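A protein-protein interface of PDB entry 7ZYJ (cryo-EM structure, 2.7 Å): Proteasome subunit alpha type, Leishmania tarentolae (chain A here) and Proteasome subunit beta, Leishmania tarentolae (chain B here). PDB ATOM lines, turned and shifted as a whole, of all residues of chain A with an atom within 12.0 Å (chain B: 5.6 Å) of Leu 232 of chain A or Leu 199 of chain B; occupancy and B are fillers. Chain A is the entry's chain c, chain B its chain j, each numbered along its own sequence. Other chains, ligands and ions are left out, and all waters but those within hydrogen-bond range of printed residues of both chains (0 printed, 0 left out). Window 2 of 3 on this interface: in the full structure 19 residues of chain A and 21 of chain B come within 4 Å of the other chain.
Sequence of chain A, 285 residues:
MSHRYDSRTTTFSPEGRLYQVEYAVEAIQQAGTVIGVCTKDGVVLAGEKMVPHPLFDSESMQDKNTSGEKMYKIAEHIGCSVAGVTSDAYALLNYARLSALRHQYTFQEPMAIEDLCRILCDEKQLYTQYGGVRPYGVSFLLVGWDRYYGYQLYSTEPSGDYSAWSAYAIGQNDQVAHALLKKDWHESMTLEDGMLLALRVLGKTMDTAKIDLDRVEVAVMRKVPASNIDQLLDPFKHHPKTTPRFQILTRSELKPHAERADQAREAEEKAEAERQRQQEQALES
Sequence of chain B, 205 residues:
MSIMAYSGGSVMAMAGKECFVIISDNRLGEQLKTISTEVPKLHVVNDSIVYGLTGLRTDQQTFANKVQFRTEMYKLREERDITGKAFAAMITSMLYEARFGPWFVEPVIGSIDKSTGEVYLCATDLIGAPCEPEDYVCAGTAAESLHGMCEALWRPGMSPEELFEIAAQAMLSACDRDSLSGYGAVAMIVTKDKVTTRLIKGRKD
OG1 of Thr 197 of chain B lies within hydrogen-bond range of OD2 of Asp 230 of chain A (3.2 Å).
The backbone NH (N) of Ala 187 of chain B lies within hydrogen-bond range of the backbone carbonyl oxygen (O) of Arg 198 of chain B (2.9 Å).
Leu 232 of chain A touches Pro 40 of chain B. CB of Leu 232 of chain A touches CG2 of Thr 197 of chain B, 3.7 Å away. Leu 232 of chain A touches Arg 198 of chain B (CD2 to C, 3.8 Å). CD2 of Leu 232 of chain A touches N of Leu 199 of chain B, 3.7 Å away. Leu 233 of chain A touches Pro 40 of chain B. CD2 of Leu 233 of chain A touches CG2 of Val 186 of chain B, 3.95 Å away.
Leu 232 of chain A touches just these residues of chain B: Pro 40 (3.7 Å), Thr 197 (3.7 Å), Arg 198 (3.8 Å) and Leu 199 (3.7 Å). Of chain A, only Leu 232 (3.7 Å) comes within 4 Å of Leu 199 of chain B. Pro 40 of chain B touches just these residues of chain A: Leu 232 and Leu 233. No residue of chain A comes within 4 Å of Ala 185 of chain B. No residue of chain A comes within 4 Å of Ile 200 of chain B. No residue of chain A comes within 4 Å of Lys 201 of chain B. Of the printed residues of chain B, Asp 230 of chain A touches Thr 197 (3.2 Å). Of the printed residues of chain A, Arg 198 of chain B touches Leu 232 (3.8 Å). Of the printed residues of chain B, Leu 233 of chain A touches Pro 40 (3.1 Å) and Val 186 (3.95 Å). The nearest residue of chain B that does not touch Leu 232 of chain A is Val 186 of chain B (4.1 Å). The nearest printed residue of chain A that does not touch Arg 198 of chain B is Asp 230 of chain A (6.7 Å).
Hydrophobic or aromatic side chains of chain A that line the printed part of chain B: Leu 232 and Leu 233. Hydrophobic or aromatic side chains of chain B within 4 Å of the printed part of chain A: Pro 40, Val 186 and Leu 199. Among the printed residues, no Asp or Glu carboxylate lies within 4 Å of a Lys or Arg side-chain nitrogen of the other chain.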
ATOM      1  N   SER A 227     -23.752 -10.487 -21.647  1.00  0.00           N
ATOM      2  CA  SER A 227     -22.634 -10.714 -22.555  1.00  0.00           C
ATOM      3  C   SER A 227     -21.545 -11.601 -21.970  1.00  0.00           C
ATOM      4  O   SER A 227     -20.944 -12.397 -22.697  1.00  0.00           O
ATOM      5  CB  SER A 227     -22.029  -9.367 -22.978  1.00  0.00           C
ATOM      6  OG  SER A 227     -20.946  -9.550 -23.873  1.00  0.00           O
ATOM      7  N   ASN A 228     -21.275 -11.492 -20.671  1.00  0.00           N
ATOM      8  CA  ASN A 228     -20.127 -12.142 -20.044  1.00  0.00           C
ATOM      9  C   ASN A 228     -20.562 -13.213 -19.045  1.00  0.00           C
ATOM     10  O   ASN A 228     -20.037 -13.304 -17.935  1.00  0.00           O
ATOM     11  CB  ASN A 228     -19.230 -11.107 -19.367  1.00  0.00           C
ATOM     12  CG  ASN A 228     -17.856 -11.655 -19.022  1.00  0.00           C
ATOM     13  OD1 ASN A 228     -17.554 -12.819 -19.283  1.00  0.00           O
ATOM     14  ND2 ASN A 228     -17.014 -10.812 -18.434  1.00  0.00           N
ATOM     15  N   ILE A 229     -21.538 -14.032 -19.427  1.00  0.00           N
ATOM     16  CA  ILE A 229     -21.994 -15.130 -18.582  1.00  0.00           C
ATOM     17  C   ILE A 229     -21.021 -16.294 -18.740  1.00  0.00           C
ATOM     18  O   ILE A 229     -20.860 -16.837 -19.834  1.00  0.00           O
ATOM     19  CB  ILE A 229     -23.425 -15.555 -18.930  1.00  0.00           C
ATOM     20  CG1 ILE A 229     -24.371 -14.357 -18.836  1.00  0.00           C
ATOM     21  CG2 ILE A 229     -23.883 -16.685 -18.021  1.00  0.00           C
ATOM     22  CD1 ILE A 229     -24.257 -13.586 -17.537  1.00  0.00           C
ATOM     23  N   ASP A 230     -20.370 -16.677 -17.644  1.00  0.00           N
ATOM     24  CA  ASP A 230     -19.461 -17.822 -17.615  1.00  0.00           C
ATOM     25  C   ASP A 230     -19.905 -18.734 -16.474  1.00  0.00           C
ATOM     26  O   ASP A 230     -19.492 -18.549 -15.324  1.00  0.00           O
ATOM     27  CB  ASP A 230     -18.013 -17.371 -17.447  1.00  0.00           C
ATOM     28  CG  ASP A 230     -17.019 -18.453 -17.824  1.00  0.00           C
ATOM     29  OD1 ASP A 230     -17.459 -19.546 -18.243  1.00  0.00           O
ATOM     30  OD2 ASP A 230     -15.800 -18.211 -17.707  1.00  0.00           O
ATOM     31  N   GLN A 231     -20.745 -19.720 -16.798  1.00  0.00           N
ATOM     32  CA  GLN A 231     -21.310 -20.587 -15.770  1.00  0.00           C
ATOM     33  C   GLN A 231     -20.286 -21.572 -15.222  1.00  0.00           C
ATOM     34  O   GLN A 231     -20.396 -21.996 -14.066  1.00  0.00           O
ATOM     35  CB  GLN A 231     -22.518 -21.339 -16.331  1.00  0.00           C
ATOM     36  CG  GLN A 231     -23.390 -22.003 -15.278  1.00  0.00           C
ATOM     37  CD  GLN A 231     -24.203 -21.009 -14.475  1.00  0.00           C
ATOM     38  OE1 GLN A 231     -25.331 -20.675 -14.840  1.00  0.00           O
ATOM     39  NE2 GLN A 231     -23.636 -20.532 -13.374  1.00  0.00           N
ATOM     40  N   LEU A 232     -19.288 -21.945 -16.026  1.00  0.00           N
ATOM     41  CA  LEU A 232     -18.320 -22.949 -15.597  1.00  0.00           C
ATOM     42  C   LEU A 232     -17.443 -22.474 -14.445  1.00  0.00           C
ATOM     43  O   LEU A 232     -16.915 -23.310 -13.705  1.00  0.00           O
ATOM     44  CB  LEU A 232     -17.437 -23.371 -16.772  1.00  0.00           C
ATOM     45  CG  LEU A 232     -17.958 -24.495 -17.669  1.00  0.00           C
ATOM     46  CD1 LEU A 232     -19.071 -23.995 -18.570  1.00  0.00           C
ATOM     47  CD2 LEU A 232     -16.828 -25.090 -18.493  1.00  0.00           C
ATOM     48  N   LEU A 233     -17.271 -21.165 -14.277  1.00  0.00           N
ATOM     49  CA  LEU A 233     -16.424 -20.646 -13.212  1.00  0.00           C
ATOM     50  C   LEU A 233     -17.110 -20.612 -11.854  1.00  0.00           C
ATOM     51  O   LEU A 233     -16.424 -20.470 -10.837  1.00  0.00           O
ATOM     52  CB  LEU A 233     -15.932 -19.239 -13.557  1.00  0.00           C
ATOM     53  CG  LEU A 233     -14.909 -19.120 -14.685  1.00  0.00           C
ATOM     54  CD1 LEU A 233     -14.173 -17.803 -14.558  1.00  0.00           C
ATOM     55  CD2 LEU A 233     -13.933 -20.283 -14.664  1.00  0.00           C
ATOM     56  N   ASP A 234     -18.434 -20.721 -11.807  1.00  0.00           N
ATOM     57  CA  ASP A 234     -19.158 -20.870 -10.544  1.00  0.00           C
ATOM     58  C   ASP A 234     -20.510 -21.484 -10.863  1.00  0.00           C
ATOM     59  O   ASP A 234     -21.499 -20.776 -11.095  1.00  0.00           O
ATOM     60  CB  ASP A 234     -19.308 -19.532  -9.822  1.00  0.00           C
ATOM     61  CG  ASP A 234     -19.916 -19.681  -8.443  1.00  0.00           C
ATOM     62  OD1 ASP A 234     -19.205 -20.149  -7.531  1.00  0.00           O
ATOM     63  OD2 ASP A 234     -21.100 -19.350  -8.260  1.00  0.00           O
ATOM     64  N   PRO A 235     -20.588 -22.816 -10.896  1.00  0.00           N
ATOM     65  CA  PRO A 235     -21.776 -23.485 -11.449  1.00  0.00           C
ATOM     66  C   PRO A 235     -23.067 -23.216 -10.690  1.00  0.00           C
ATOM     67  O   PRO A 235     -24.157 -23.447 -11.223  1.00  0.00           O
ATOM     68  CB  PRO A 235     -21.399 -24.972 -11.382  1.00  0.00           C
ATOM     69  CG  PRO A 235     -19.901 -24.990 -11.288  1.00  0.00           C
ATOM     70  CD  PRO A 235     -19.540 -23.773 -10.509  1.00  0.00           C
ATOM     71  N   PHE A 236     -22.970 -22.729  -9.454  1.00  0.00           N
ATOM     72  CA  PHE A 236     -24.141 -22.534  -8.613  1.00  0.00           C
ATOM     73  C   PHE A 236     -24.692 -21.115  -8.645  1.00  0.00           C
ATOM     74  O   PHE A 236     -25.692 -20.843  -7.969  1.00  0.00           O
ATOM     75  CB  PHE A 236     -23.817 -22.922  -7.164  1.00  0.00           C
ATOM     76  CG  PHE A 236     -23.594 -24.395  -6.965  1.00  0.00           C
ATOM     77  CD1 PHE A 236     -24.658 -25.243  -6.702  1.00  0.00           C
ATOM     78  CD2 PHE A 236     -22.320 -24.930  -7.039  1.00  0.00           C
ATOM     79  CE1 PHE A 236     -24.452 -26.597  -6.518  1.00  0.00           C
ATOM     80  CE2 PHE A 236     -22.107 -26.284  -6.857  1.00  0.00           C
ATOM     81  CZ  PHE A 236     -23.175 -27.118  -6.597  1.00  0.00           C
ATOM     82  N   LYS A 237     -24.087 -20.206  -9.405  1.00  0.00           N
ATOM     83  CA  LYS A 237     -24.535 -18.819  -9.448  1.00  0.00           C
ATOM     84  C   LYS A 237     -25.514 -18.642 -10.601  1.00  0.00           C
ATOM     85  O   LYS A 237     -25.196 -18.967 -11.750  1.00  0.00           O
ATOM     86  CB  LYS A 237     -23.351 -17.865  -9.600  1.00  0.00           C
ATOM     87  CG  LYS A 237     -23.631 -16.434  -9.164  1.00  0.00           C
ATOM     88  CD  LYS A 237     -24.078 -15.565 -10.322  1.00  0.00           C
ATOM     89  CE  LYS A 237     -24.292 -14.128  -9.877  1.00  0.00           C
ATOM     90  NZ  LYS A 237     -24.795 -13.268 -10.984  1.00  0.00           N
ATOM     91  N   HIS A 238     -26.703 -18.137 -10.290  1.00  0.00           N
ATOM     92  CA  HIS A 238     -27.698 -17.835 -11.309  1.00  0.00           C
ATOM     93  C   HIS A 238     -27.335 -16.535 -12.014  1.00  0.00           C
ATOM     94  O   HIS A 238     -27.115 -15.508 -11.363  1.00  0.00           O
ATOM     95  CB  HIS A 238     -29.086 -17.739 -10.683  1.00  0.00           C
ATOM     96  CG  HIS A 238     -30.146 -17.295 -11.640  1.00  0.00           C
ATOM     97  ND1 HIS A 238     -30.658 -18.122 -12.615  1.00  0.00           N
ATOM     98  CD2 HIS A 238     -30.796 -16.114 -11.768  1.00  0.00           C
ATOM     99  CE1 HIS A 238     -31.577 -17.469 -13.304  1.00  0.00           C
ATOM    100  NE2 HIS A 238     -31.680 -16.249 -12.811  1.00  0.00           N
ATOM    101  N   HIS A 239     -27.280 -16.578 -13.340  1.00  0.00           N
ATOM    102  CA  HIS A 239     -26.979 -15.393 -14.131  1.00  0.00           C
ATOM    103  C   HIS A 239     -28.218 -14.942 -14.883  1.00  0.00           C
ATOM    104  O   HIS A 239     -28.762 -15.717 -15.682  1.00  0.00           O
ATOM    105  CB  HIS A 239     -25.854 -15.678 -15.121  1.00  0.00           C
ATOM    106  CG  HIS A 239     -24.636 -16.282 -14.496  1.00  0.00           C
ATOM    107  ND1 HIS A 239     -23.678 -15.529 -13.853  1.00  0.00           N
ATOM    108  CD2 HIS A 239     -24.218 -17.567 -14.420  1.00  0.00           C
ATOM    109  CE1 HIS A 239     -22.723 -16.324 -13.407  1.00  0.00           C
ATOM    110  NE2 HIS A 239     -23.026 -17.566 -13.736  1.00  0.00           N
ATOM    111  N   LYS A 241     -30.695 -13.324 -17.643  1.00  0.00           N
ATOM    112  CA  LYS A 241     -30.597 -13.249 -19.095  1.00  0.00           C
ATOM    113  C   LYS A 241     -30.276 -11.841 -19.581  1.00  0.00           C
ATOM    114  O   LYS A 241     -29.512 -11.681 -20.538  1.00  0.00           O
ATOM    115  CB  LYS A 241     -31.899 -13.737 -19.737  1.00  0.00           C
ATOM    116  CG  LYS A 241     -32.288 -15.186 -19.423  1.00  0.00           C
ATOM    117  CD  LYS A 241     -31.382 -16.215 -20.102  1.00  0.00           C
ATOM    118  CE  LYS A 241     -30.233 -16.669 -19.208  1.00  0.00           C
ATOM    119  NZ  LYS A 241     -29.428 -17.746 -19.845  1.00  0.00           N
ATOM    120  N   ASN B  26     -10.938 -28.336  -8.889  1.00  0.00           N
ATOM    121  CA  ASN B  26     -12.318 -28.167  -8.463  1.00  0.00           C
ATOM    122  C   ASN B  26     -12.564 -28.504  -7.000  1.00  0.00           C
ATOM    123  O   ASN B  26     -13.668 -28.251  -6.506  1.00  0.00           O
ATOM    124  CB  ASN B  26     -13.247 -29.026  -9.333  1.00  0.00           C
ATOM    125  CG  ASN B  26     -13.412 -28.473 -10.731  1.00  0.00           C
ATOM    126  OD1 ASN B  26     -13.663 -27.283 -10.915  1.00  0.00           O
ATOM    127  ND2 ASN B  26     -13.272 -29.336 -11.728  1.00  0.00           N
ATOM    128  N   PRO B  40     -14.325 -24.243  -8.535  1.00  0.00           N
ATOM    129  CA  PRO B  40     -13.182 -23.638  -9.223  1.00  0.00           C
ATOM    130  C   PRO B  40     -12.696 -22.386  -8.506  1.00  0.00           C
ATOM    131  O   PRO B  40     -13.431 -21.733  -7.763  1.00  0.00           O
ATOM    132  CB  PRO B  40     -13.735 -23.301 -10.612  1.00  0.00           C
ATOM    133  CG  PRO B  40     -15.214 -23.349 -10.475  1.00  0.00           C
ATOM    134  CD  PRO B  40     -15.513 -24.327  -9.397  1.00  0.00           C
ATOM    135  N   ALA B 185     -10.830 -30.455 -13.676  1.00  0.00           N
ATOM    136  CA  ALA B 185     -10.226 -29.133 -13.741  1.00  0.00           C
ATOM    137  C   ALA B 185     -11.115 -28.210 -14.558  1.00  0.00           C
ATOM    138  O   ALA B 185     -12.010 -28.652 -15.280  1.00  0.00           O
ATOM    139  CB  ALA B 185      -8.814 -29.192 -14.335  1.00  0.00           C
ATOM    140  N   VAL B 186     -10.860 -26.913 -14.433  1.00  0.00           N
ATOM    141  CA  VAL B 186     -11.492 -25.904 -15.274  1.00  0.00           C
ATOM    142  C   VAL B 186     -10.393 -25.031 -15.863  1.00  0.00           C
ATOM    143  O   VAL B 186      -9.493 -24.585 -15.144  1.00  0.00           O
ATOM    144  CB  VAL B 186     -12.526 -25.063 -14.497  1.00  0.00           C
ATOM    145  CG1 VAL B 186     -11.872 -24.315 -13.352  1.00  0.00           C
ATOM    146  CG2 VAL B 186     -13.236 -24.099 -15.432  1.00  0.00           C
ATOM    147  N   ALA B 187     -10.447 -24.817 -17.173  1.00  0.00           N
ATOM    148  CA  ALA B 187      -9.410 -24.091 -17.883  1.00  0.00           C
ATOM    149  C   ALA B 187     -10.013 -22.939 -18.673  1.00  0.00           C
ATOM    150  O   ALA B 187     -11.151 -23.010 -19.146  1.00  0.00           O
ATOM    151  CB  ALA B 187      -8.631 -25.014 -18.826  1.00  0.00           C
ATOM    152  N   THR B 197     -13.741 -21.216 -22.410  1.00  0.00           N
ATOM    153  CA  THR B 197     -13.797 -21.883 -21.118  1.00  0.00           C
ATOM    154  C   THR B 197     -14.094 -23.359 -21.330  1.00  0.00           C
ATOM    155  O   THR B 197     -15.015 -23.716 -22.072  1.00  0.00           O
ATOM    156  CB  THR B 197     -14.861 -21.257 -20.213  1.00  0.00           C
ATOM    157  OG1 THR B 197     -14.694 -19.835 -20.191  1.00  0.00           O
ATOM    158  CG2 THR B 197     -14.737 -21.797 -18.797  1.00  0.00           C
ATOM    159  N   ARG B 198     -13.311 -24.217 -20.681  1.00  0.00           N
ATOM    160  CA  ARG B 198     -13.445 -25.657 -20.840  1.00  0.00           C
ATOM    161  C   ARG B 198     -13.405 -26.323 -19.475  1.00  0.00           C
ATOM    162  O   ARG B 198     -12.784 -25.805 -18.543  1.00  0.00           O
ATOM    163  CB  ARG B 198     -12.335 -26.224 -21.733  1.00  0.00           C
ATOM    164  CG  ARG B 198     -12.419 -25.777 -23.183  1.00  0.00           C
ATOM    165  CD  ARG B 198     -11.295 -26.364 -24.021  1.00  0.00           C
ATOM    166  NE  ARG B 198     -11.369 -25.914 -25.405  1.00  0.00           N
ATOM    167  CZ  ARG B 198     -10.487 -26.225 -26.345  1.00  0.00           C
ATOM    168  NH1 ARG B 198      -9.446 -26.999 -26.088  1.00  0.00           N
ATOM    169  NH2 ARG B 198     -10.656 -25.749 -27.575  1.00  0.00           N
ATOM    170  N   LEU B 199     -14.077 -27.462 -19.356  1.00  0.00           N
ATOM    171  CA  LEU B 199     -14.035 -28.275 -18.149  1.00  0.00           C
ATOM    172  C   LEU B 199     -13.425 -29.622 -18.512  1.00  0.00           C
ATOM    173  O   LEU B 199     -13.852 -30.260 -19.478  1.00  0.00           O
ATOM    174  CB  LEU B 199     -15.433 -28.446 -17.548  1.00  0.00           C
ATOM    175  CG  LEU B 199     -15.544 -28.975 -16.113  1.00  0.00           C
ATOM    176  CD1 LEU B 199     -16.840 -28.490 -15.486  1.00  0.00           C
ATOM    177  CD2 LEU B 199     -15.446 -30.487 -16.027  1.00  0.00           C
ATOM    178  N   ILE B 200     -12.432 -30.049 -17.738  1.00  0.00           N
ATOM    179  CA  ILE B 200     -11.562 -31.161 -18.098  1.00  0.00           C
ATOM    180  C   ILE B 200     -11.821 -32.315 -17.140  1.00  0.00           C
ATOM    181  O   ILE B 200     -11.802 -32.133 -15.914  1.00  0.00           O
ATOM    182  CB  ILE B 200     -10.085 -30.745 -18.073  1.00  0.00           C
ATOM    183  CG1 ILE B 200      -9.897 -29.451 -18.865  1.00  0.00           C
ATOM    184  CG2 ILE B 200      -9.209 -31.849 -18.640  1.00  0.00           C
ATOM    185  CD1 ILE B 200      -8.572 -28.785 -18.632  1.00  0.00           C
ATOM    186  N   LYS B 201     -12.054 -33.497 -17.712  1.00  0.00           N
ATOM    187  CA  LYS B 201     -12.285 -34.709 -16.938  1.00  0.00           C
ATOM    188  C   LYS B 201     -11.107 -34.993 -16.018  1.00  0.00           C
ATOM    189  O   LYS B 201      -9.948 -34.820 -16.403  1.00  0.00           O
ATOM    190  CB  LYS B 201     -12.491 -35.901 -17.873  1.00  0.00           C
ATOM    191  CG  LYS B 201     -13.680 -35.815 -18.812  1.00  0.00           C
ATOM    192  CD  LYS B 201     -14.999 -35.904 -18.076  1.00  0.00           C
ATOM    193  CE  LYS B 201     -16.158 -35.811 -19.052  1.00  0.00           C
ATOM    194  NZ  LYS B 201     -16.231 -37.007 -19.934  1.00  0.00           N
